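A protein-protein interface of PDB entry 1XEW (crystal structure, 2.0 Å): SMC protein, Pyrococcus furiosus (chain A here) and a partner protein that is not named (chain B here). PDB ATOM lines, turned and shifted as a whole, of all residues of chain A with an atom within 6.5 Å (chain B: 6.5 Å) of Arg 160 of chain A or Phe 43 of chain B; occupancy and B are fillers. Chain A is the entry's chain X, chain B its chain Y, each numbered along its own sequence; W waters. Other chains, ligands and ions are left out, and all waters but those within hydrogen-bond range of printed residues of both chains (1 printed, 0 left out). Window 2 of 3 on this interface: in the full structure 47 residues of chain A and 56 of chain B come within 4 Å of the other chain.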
ATOM      1  N   SER A 155     -18.313 -18.658 -32.030  1.00  0.00           N
ATOM      2  CA  SER A 155     -16.999 -18.456 -31.408  1.00  0.00           C
ATOM      3  C   SER A 155     -16.599 -19.862 -30.983  1.00  0.00           C
ATOM      4  O   SER A 155     -17.474 -20.739 -30.824  1.00  0.00           O
ATOM      5  CB  SER A 155     -17.097 -17.609 -30.166  1.00  0.00           C
ATOM      6  OG  SER A 155     -17.679 -18.412 -29.103  1.00  0.00           O
ATOM      7  N   PRO A 156     -15.299 -20.107 -30.782  1.00  0.00           N
ATOM      8  CA  PRO A 156     -14.920 -21.465 -30.384  1.00  0.00           C
ATOM      9  C   PRO A 156     -15.507 -21.873 -29.043  1.00  0.00           C
ATOM     10  O   PRO A 156     -15.745 -23.033 -28.832  1.00  0.00           O
ATOM     11  CB  PRO A 156     -13.382 -21.406 -30.376  1.00  0.00           C
ATOM     12  CG  PRO A 156     -13.087 -20.522 -31.564  1.00  0.00           C
ATOM     13  CD  PRO A 156     -14.152 -19.366 -31.373  1.00  0.00           C
ATOM     14  N   LEU A 157     -15.735 -20.892 -28.160  1.00  0.00           N
ATOM     15  CA  LEU A 157     -16.322 -21.140 -26.839  1.00  0.00           C
ATOM     16  C   LEU A 157     -17.757 -21.645 -27.038  1.00  0.00           C
ATOM     17  O   LEU A 157     -18.188 -22.682 -26.431  1.00  0.00           O
ATOM     18  CB  LEU A 157     -16.354 -19.834 -26.017  1.00  0.00           C
ATOM     19  CG  LEU A 157     -16.137 -19.947 -24.496  1.00  0.00           C
ATOM     20  CD1 LEU A 157     -16.732 -18.672 -23.755  1.00  0.00           C
ATOM     21  CD2 LEU A 157     -16.628 -21.355 -23.915  1.00  0.00           C
ATOM     22  N   GLU A 158     -18.559 -20.888 -27.816  1.00  0.00           N
ATOM     23  CA  GLU A 158     -19.924 -21.372 -28.043  1.00  0.00           C
ATOM     24  C   GLU A 158     -19.930 -22.780 -28.677  1.00  0.00           C
ATOM     25  O   GLU A 158     -20.734 -23.672 -28.315  1.00  0.00           O
ATOM     26  CB  GLU A 158     -20.745 -20.432 -28.976  1.00  0.00           C
ATOM     27  CG  GLU A 158     -22.264 -20.865 -28.911  1.00  0.00           C
ATOM     28  CD  GLU A 158     -23.165 -20.059 -29.821  1.00  0.00           C
ATOM     29  OE1 GLU A 158     -22.917 -18.837 -30.024  1.00  0.00           O
ATOM     30  OE2 GLU A 158     -24.129 -20.642 -30.323  1.00  0.00           O
ATOM     31  N   ARG A 159     -18.998 -23.015 -29.604  1.00  0.00           N
ATOM     32  CA  ARG A 159     -18.954 -24.340 -30.229  1.00  0.00           C
ATOM     33  C   ARG A 159     -18.670 -25.427 -29.168  1.00  0.00           C
ATOM     34  O   ARG A 159     -19.268 -26.471 -29.239  1.00  0.00           O
ATOM     35  CB  ARG A 159     -17.933 -24.333 -31.374  1.00  0.00           C
ATOM     36  CG  ARG A 159     -17.899 -25.597 -32.124  1.00  0.00           C
ATOM     37  CD  ARG A 159     -17.050 -25.522 -33.354  1.00  0.00           C
ATOM     38  NE  ARG A 159     -17.425 -24.546 -34.363  1.00  0.00           N
ATOM     39  CZ  ARG A 159     -16.782 -23.419 -34.633  1.00  0.00           C
ATOM     40  NH1 ARG A 159     -17.233 -22.619 -35.615  1.00  0.00           N
ATOM     41  NH2 ARG A 159     -15.691 -23.099 -33.941  1.00  0.00           N
ATOM     42  N   ARG A 160     -17.815 -25.186 -28.164  1.00  0.00           N
ATOM     43  CA  ARG A 160     -17.577 -26.235 -27.138  1.00  0.00           C
ATOM     44  C   ARG A 160     -18.838 -26.334 -26.248  1.00  0.00           C
ATOM     45  O   ARG A 160     -19.233 -27.407 -25.798  1.00  0.00           O
ATOM     46  CB  ARG A 160     -16.337 -25.898 -26.228  1.00  0.00           C
ATOM     47  CG  ARG A 160     -15.881 -27.084 -25.328  1.00  0.00           C
ATOM     48  CD  ARG A 160     -16.312 -26.904 -23.784  1.00  0.00           C
ATOM     49  NE  ARG A 160     -15.738 -25.689 -23.294  1.00  0.00           N
ATOM     50  CZ  ARG A 160     -16.280 -24.814 -22.463  1.00  0.00           C
ATOM     51  NH1 ARG A 160     -15.546 -23.758 -22.160  1.00  0.00           N
ATOM     52  NH2 ARG A 160     -17.498 -24.967 -21.939  1.00  0.00           N
ATOM     53  N   LEU A 161     -19.487 -25.189 -25.975  1.00  0.00           N
ATOM     54  CA  LEU A 161     -20.732 -25.227 -25.180  1.00  0.00           C
ATOM     55  C   LEU A 161     -21.830 -26.115 -25.836  1.00  0.00           C
ATOM     56  O   LEU A 161     -22.588 -26.799 -25.121  1.00  0.00           O
ATOM     57  CB  LEU A 161     -21.257 -23.779 -24.959  1.00  0.00           C
ATOM     58  CG  LEU A 161     -20.372 -22.900 -24.055  1.00  0.00           C
ATOM     59  CD1 LEU A 161     -20.837 -21.397 -24.050  1.00  0.00           C
ATOM     60  CD2 LEU A 161     -20.447 -23.475 -22.670  1.00  0.00           C
ATOM     61  N   LEU A 162     -21.944 -26.133 -27.179  1.00  0.00           N
ATOM     62  CA  LEU A 162     -22.974 -27.033 -27.819  1.00  0.00           C
ATOM     63  C   LEU A 162     -22.602 -28.465 -27.491  1.00  0.00           C
ATOM     64  O   LEU A 162     -23.499 -29.326 -27.235  1.00  0.00           O
ATOM     65  CB  LEU A 162     -22.978 -26.970 -29.333  1.00  0.00           C
ATOM     66  CG  LEU A 162     -23.160 -25.570 -29.894  1.00  0.00           C
ATOM     67  CD1 LEU A 162     -23.108 -25.621 -31.459  1.00  0.00           C
ATOM     68  CD2 LEU A 162     -24.508 -25.001 -29.345  1.00  0.00           C
ATOM     69  N   ILE A 163     -21.275 -28.742 -27.480  1.00  0.00           N
ATOM     70  CA  ILE A 163     -20.918 -30.110 -27.180  1.00  0.00           C
ATOM     71  C   ILE A 163     -21.237 -30.365 -25.713  1.00  0.00           C
ATOM     72  O   ILE A 163     -21.774 -31.388 -25.409  1.00  0.00           O
ATOM     73  CB  ILE A 163     -19.388 -30.466 -27.449  1.00  0.00           C
ATOM     74  CG1 ILE A 163     -18.938 -29.975 -28.848  1.00  0.00           C
ATOM     75  CG2 ILE A 163     -19.192 -31.940 -27.214  1.00  0.00           C
ATOM     76  CD1 ILE A 163     -19.869 -30.303 -30.035  1.00  0.00           C
ATOM     77  N   ASP A 164     -20.975 -29.431 -24.812  1.00  0.00           N
ATOM     78  CA  ASP A 164     -21.330 -29.727 -23.355  1.00  0.00           C
ATOM     79  C   ASP A 164     -22.827 -30.141 -23.216  1.00  0.00           C
ATOM     80  O   ASP A 164     -23.151 -31.139 -22.553  1.00  0.00           O
ATOM     81  CB  ASP A 164     -21.156 -28.532 -22.390  1.00  0.00           C
ATOM     82  CG  ASP A 164     -19.703 -28.001 -22.249  1.00  0.00           C
ATOM     83  OD1 ASP A 164     -19.483 -27.195 -21.310  1.00  0.00           O
ATOM     84  OD2 ASP A 164     -18.768 -28.290 -23.038  1.00  0.00           O
ATOM     85  N   ASP A 165     -23.720 -29.335 -23.840  1.00  0.00           N
ATOM     86  CA  ASP A 165     -25.177 -29.543 -23.758  1.00  0.00           C
ATOM     87  C   ASP A 165     -25.600 -30.870 -24.345  1.00  0.00           C
ATOM     88  O   ASP A 165     -26.427 -31.550 -23.735  1.00  0.00           O
ATOM     89  CB  ASP A 165     -25.964 -28.421 -24.468  1.00  0.00           C
ATOM     90  CG  ASP A 165     -25.752 -27.046 -23.831  1.00  0.00           C
ATOM     91  OD1 ASP A 165     -26.170 -26.054 -24.468  1.00  0.00           O
ATOM     92  OD2 ASP A 165     -25.172 -26.947 -22.719  1.00  0.00           O
ATOM     93  N   PHE B   8     -17.892 -35.627 -21.165  1.00  0.00           N
ATOM     94  CA  PHE B   8     -17.766 -34.593 -22.210  1.00  0.00           C
ATOM     95  C   PHE B   8     -16.880 -35.206 -23.292  1.00  0.00           C
ATOM     96  O   PHE B   8     -17.204 -35.206 -24.477  1.00  0.00           O
ATOM     97  CB  PHE B   8     -17.032 -33.342 -21.709  1.00  0.00           C
ATOM     98  CG  PHE B   8     -16.642 -32.405 -22.827  1.00  0.00           C
ATOM     99  CD1 PHE B   8     -17.538 -31.418 -23.295  1.00  0.00           C
ATOM    100  CD2 PHE B   8     -15.397 -32.530 -23.451  1.00  0.00           C
ATOM    101  CE1 PHE B   8     -17.186 -30.582 -24.348  1.00  0.00           C
ATOM    102  CE2 PHE B   8     -15.018 -31.712 -24.521  1.00  0.00           C
ATOM    103  CZ  PHE B   8     -15.928 -30.714 -24.978  1.00  0.00           C
ATOM    104  N   MET B   9     -15.773 -35.796 -22.846  1.00  0.00           N
ATOM    105  CA  MET B   9     -14.818 -36.381 -23.757  1.00  0.00           C
ATOM    106  C   MET B   9     -15.331 -37.550 -24.605  1.00  0.00           C
ATOM    107  O   MET B   9     -14.976 -37.684 -25.794  1.00  0.00           O
ATOM    108  CB  MET B   9     -13.508 -36.715 -22.977  1.00  0.00           C
ATOM    109  CG  MET B   9     -12.758 -35.455 -22.365  1.00  0.00           C
ATOM    110  SD  MET B   9     -12.352 -34.013 -23.485  1.00  0.00           S
ATOM    111  CE  MET B   9     -11.803 -34.822 -24.988  1.00  0.00           C
ATOM    112  N   LEU B  36      -9.781 -29.130 -29.470  1.00  0.00           N
ATOM    113  CA  LEU B  36     -10.023 -28.431 -28.192  1.00  0.00           C
ATOM    114  C   LEU B  36      -8.942 -27.375 -27.930  1.00  0.00           C
ATOM    115  O   LEU B  36      -7.744 -27.643 -28.120  1.00  0.00           O
ATOM    116  CB  LEU B  36     -10.021 -29.421 -27.044  1.00  0.00           C
ATOM    117  CG  LEU B  36     -11.291 -30.284 -27.058  1.00  0.00           C
ATOM    118  CD1 LEU B  36     -11.201 -31.320 -25.915  1.00  0.00           C
ATOM    119  CD2 LEU B  36     -12.538 -29.366 -26.823  1.00  0.00           C
ATOM    120  N   ASN B  38      -8.106 -26.262 -25.140  1.00  0.00           N
ATOM    121  CA  ASN B  38      -7.427 -26.645 -23.924  1.00  0.00           C
ATOM    122  C   ASN B  38      -7.687 -28.121 -23.684  1.00  0.00           C
ATOM    123  O   ASN B  38      -8.457 -28.459 -22.805  1.00  0.00           O
ATOM    124  CB  ASN B  38      -8.001 -25.892 -22.750  1.00  0.00           C
ATOM    125  CG  ASN B  38      -6.951 -25.343 -21.847  1.00  0.00           C
ATOM    126  OD1 ASN B  38      -6.777 -24.101 -21.755  1.00  0.00           O
ATOM    127  ND2 ASN B  38      -6.239 -26.238 -21.157  1.00  0.00           N
ATOM    128  N   ASP B  41      -7.723 -29.055 -19.749  1.00  0.00           N
ATOM    129  CA  ASP B  41      -8.886 -28.484 -19.014  1.00  0.00           C
ATOM    130  C   ASP B  41      -9.925 -28.021 -20.150  1.00  0.00           C
ATOM    131  O   ASP B  41     -10.155 -26.821 -20.366  1.00  0.00           O
ATOM    132  CB  ASP B  41      -8.308 -27.268 -18.223  1.00  0.00           C
ATOM    133  CG  ASP B  41      -9.220 -26.753 -17.112  1.00  0.00           C
ATOM    134  OD1 ASP B  41      -8.731 -25.951 -16.231  1.00  0.00           O
ATOM    135  OD2 ASP B  41     -10.427 -27.119 -17.128  1.00  0.00           O
ATOM    136  N   PRO B  42     -10.576 -28.971 -20.825  1.00  0.00           N
ATOM    137  CA  PRO B  42     -11.510 -28.578 -21.907  1.00  0.00           C
ATOM    138  C   PRO B  42     -12.513 -27.477 -21.621  1.00  0.00           C
ATOM    139  O   PRO B  42     -12.675 -26.601 -22.462  1.00  0.00           O
ATOM    140  CB  PRO B  42     -12.169 -29.893 -22.314  1.00  0.00           C
ATOM    141  CG  PRO B  42     -11.083 -30.944 -21.911  1.00  0.00           C
ATOM    142  CD  PRO B  42     -10.664 -30.433 -20.575  1.00  0.00           C
ATOM    143  N   PHE B  43     -13.105 -27.470 -20.423  1.00  0.00           N
ATOM    144  CA  PHE B  43     -14.111 -26.426 -20.041  1.00  0.00           C
ATOM    145  C   PHE B  43     -13.595 -24.992 -19.892  1.00  0.00           C
ATOM    146  O   PHE B  43     -14.393 -24.058 -19.793  1.00  0.00           O
ATOM    147  CB  PHE B  43     -14.822 -26.853 -18.759  1.00  0.00           C
ATOM    148  CG  PHE B  43     -15.343 -28.232 -18.836  1.00  0.00           C
ATOM    149  CD1 PHE B  43     -16.264 -28.587 -19.851  1.00  0.00           C
ATOM    150  CD2 PHE B  43     -14.817 -29.229 -18.026  1.00  0.00           C
ATOM    151  CE1 PHE B  43     -16.628 -29.907 -20.041  1.00  0.00           C
ATOM    152  CE2 PHE B  43     -15.181 -30.564 -18.210  1.00  0.00           C
ATOM    153  CZ  PHE B  43     -16.084 -30.907 -19.215  1.00  0.00           C
ATOM    154  N   SER B  44     -12.260 -24.808 -19.939  1.00  0.00           N
ATOM    155  CA  SER B  44     -11.684 -23.470 -19.849  1.00  0.00           C
ATOM    156  C   SER B  44     -11.289 -22.953 -21.267  1.00  0.00           C
ATOM    157  O   SER B  44     -10.760 -21.850 -21.409  1.00  0.00           O
ATOM    158  CB  SER B  44     -10.471 -23.485 -18.908  1.00  0.00           C
ATOM    159  OG  SER B  44      -9.353 -24.046 -19.567  1.00  0.00           O
ATOM    160  N   GLY B  45     -11.506 -23.755 -22.313  1.00  0.00           N
ATOM    161  CA  GLY B  45     -11.199 -23.242 -23.636  1.00  0.00           C
ATOM    162  C   GLY B  45     -12.343 -23.467 -24.652  1.00  0.00           C
ATOM    163  O   GLY B  45     -13.392 -24.010 -24.309  1.00  0.00           O
ATOM    164  N   GLY B  46     -12.121 -23.092 -25.905  1.00  0.00           N
ATOM    165  CA  GLY B  46     -13.160 -23.293 -26.916  1.00  0.00           C
ATOM    166  C   GLY B  46     -12.891 -24.557 -27.722  1.00  0.00           C
ATOM    167  O   GLY B  46     -12.106 -25.413 -27.257  1.00  0.00           O
ATOM    168  N   LEU B  47     -13.521 -24.667 -28.911  1.00  0.00           N
ATOM    169  CA  LEU B  47     -13.375 -25.799 -29.816  1.00  0.00           C
ATOM    170  C   LEU B  47     -13.319 -25.181 -31.220  1.00  0.00           C
ATOM    171  O   LEU B  47     -14.319 -24.589 -31.717  1.00  0.00           O
ATOM    172  CB  LEU B  47     -14.595 -26.761 -29.698  1.00  0.00           C
ATOM    173  CG  LEU B  47     -14.710 -28.045 -30.539  1.00  0.00           C
ATOM    174  CD1 LEU B  47     -15.891 -28.850 -30.148  1.00  0.00           C
ATOM    175  CD2 LEU B  47     -14.882 -27.768 -31.929  1.00  0.00           C
HETATM  176  O   HOH W   1     -16.970 -21.996 -20.663  1.00  0.00           O
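O of Pro 156 of chain A sits at hydrogen-bond distance from N of Leu 47 of chain B (2.8 Å). The backbone carbonyl oxygen (O) of Gly 45 of chain B lies within hydrogen-bond range of the guanidinium group (NH1) of Arg 160 of chain A (3.1 Å). NH1 of Arg 160 of chain A is in hydrogen-bond range of O of Phe 43 of chain B. NE of Arg 160 of chain A is in hydrogen-bond range of O of Pro 42 of chain B. NH2 of Arg 159 of chain A sits at hydrogen-bond distance from O of Leu 47 of chain B (3.0 Å).
The backbone NH (N) of Leu 157 of chain A sits close to the side-chain hydroxyl (OG) of Ser 155 of chain A (3.3 Å). NH2 of Arg 160 of chain A lies within salt-bridge range of OD1 of Asp 164 of chain A, 3.0 Å away.
CA of Gly 46 of chain B touches O of Pro 156 of chain A, at 3.2 Å. N of Leu 157 of chain A touches CA of Gly 46 of chain B (3.7 Å). CZ of Phe 8 of chain B touches CG of Arg 160 of chain A, at 3.6 Å. Gly 46 of chain B touches Arg 160 of chain A. N of Arg 160 of chain A touches CB of Leu 47 of chain B, at 3.9 Å. Ile 163 of chain A touches Phe 8 of chain B (CG2 to CE1, 3.8 Å). CG1 of Ile 163 of chain A touches CD1 of Leu 47 of chain B, at 3.5 Å. Asp 164 of chain A touches Phe 8 of chain B. CD1 of Phe 43 of chain B touches OD1 of Asp 164 of chain A, at 3.8 Å.
Of the printed residues of chain B, Arg 160 of chain A touches Phe 8 (3.6 Å), Pro 42 (3.3 Å), Phe 43 (2.6 Å), Gly 45 (3.1 Å), Gly 46 (3.99 Å) and Leu 47 (3.9 Å). Of the printed residues of chain B, Ile 163 of chain A touches Phe 8 and Leu 47. Asn 38 of chain B touches none of the printed residues of chain A. Asp 41 of chain B touches none of the printed residues of chain A. Phe 43 of chain B touches just these residues of chain A: Arg 160 (2.6 Å) and Asp 164 (3.8 Å). Of the printed residues of chain A, Gly 45 of chain B touches Arg 160 (3.1 Å). The nearest printed residue of chain B that does not touch Arg 160 of chain A is Ser 44 of chain B (4.1 Å). The nearest residue of chain A that does not touch Phe 43 of chain B is Leu 157 of chain A (5.4 Å). The nearest printed residue of chain B that does not touch Leu 157 of chain A is Gly 45 of chain B (4.2 Å).
Of the 11 printed residues of chain B, 6 touch a printed residue of chain A. Hydrophobic or aromatic side chains of chain B within 4 Å of the printed part of chain A: Phe 8, Phe 43 and Leu 47. Among the printed residues, no Asp or Glu carboxylate lies within 4 Å of a Lys or Arg side-chain nitrogen of the other chain.
Water W1 bridges the guanidinium group of Arg 160 of chain A (2.7 Å) and the backbone carbonyl oxygen of Phe 43 of chain B (3.4 Å).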
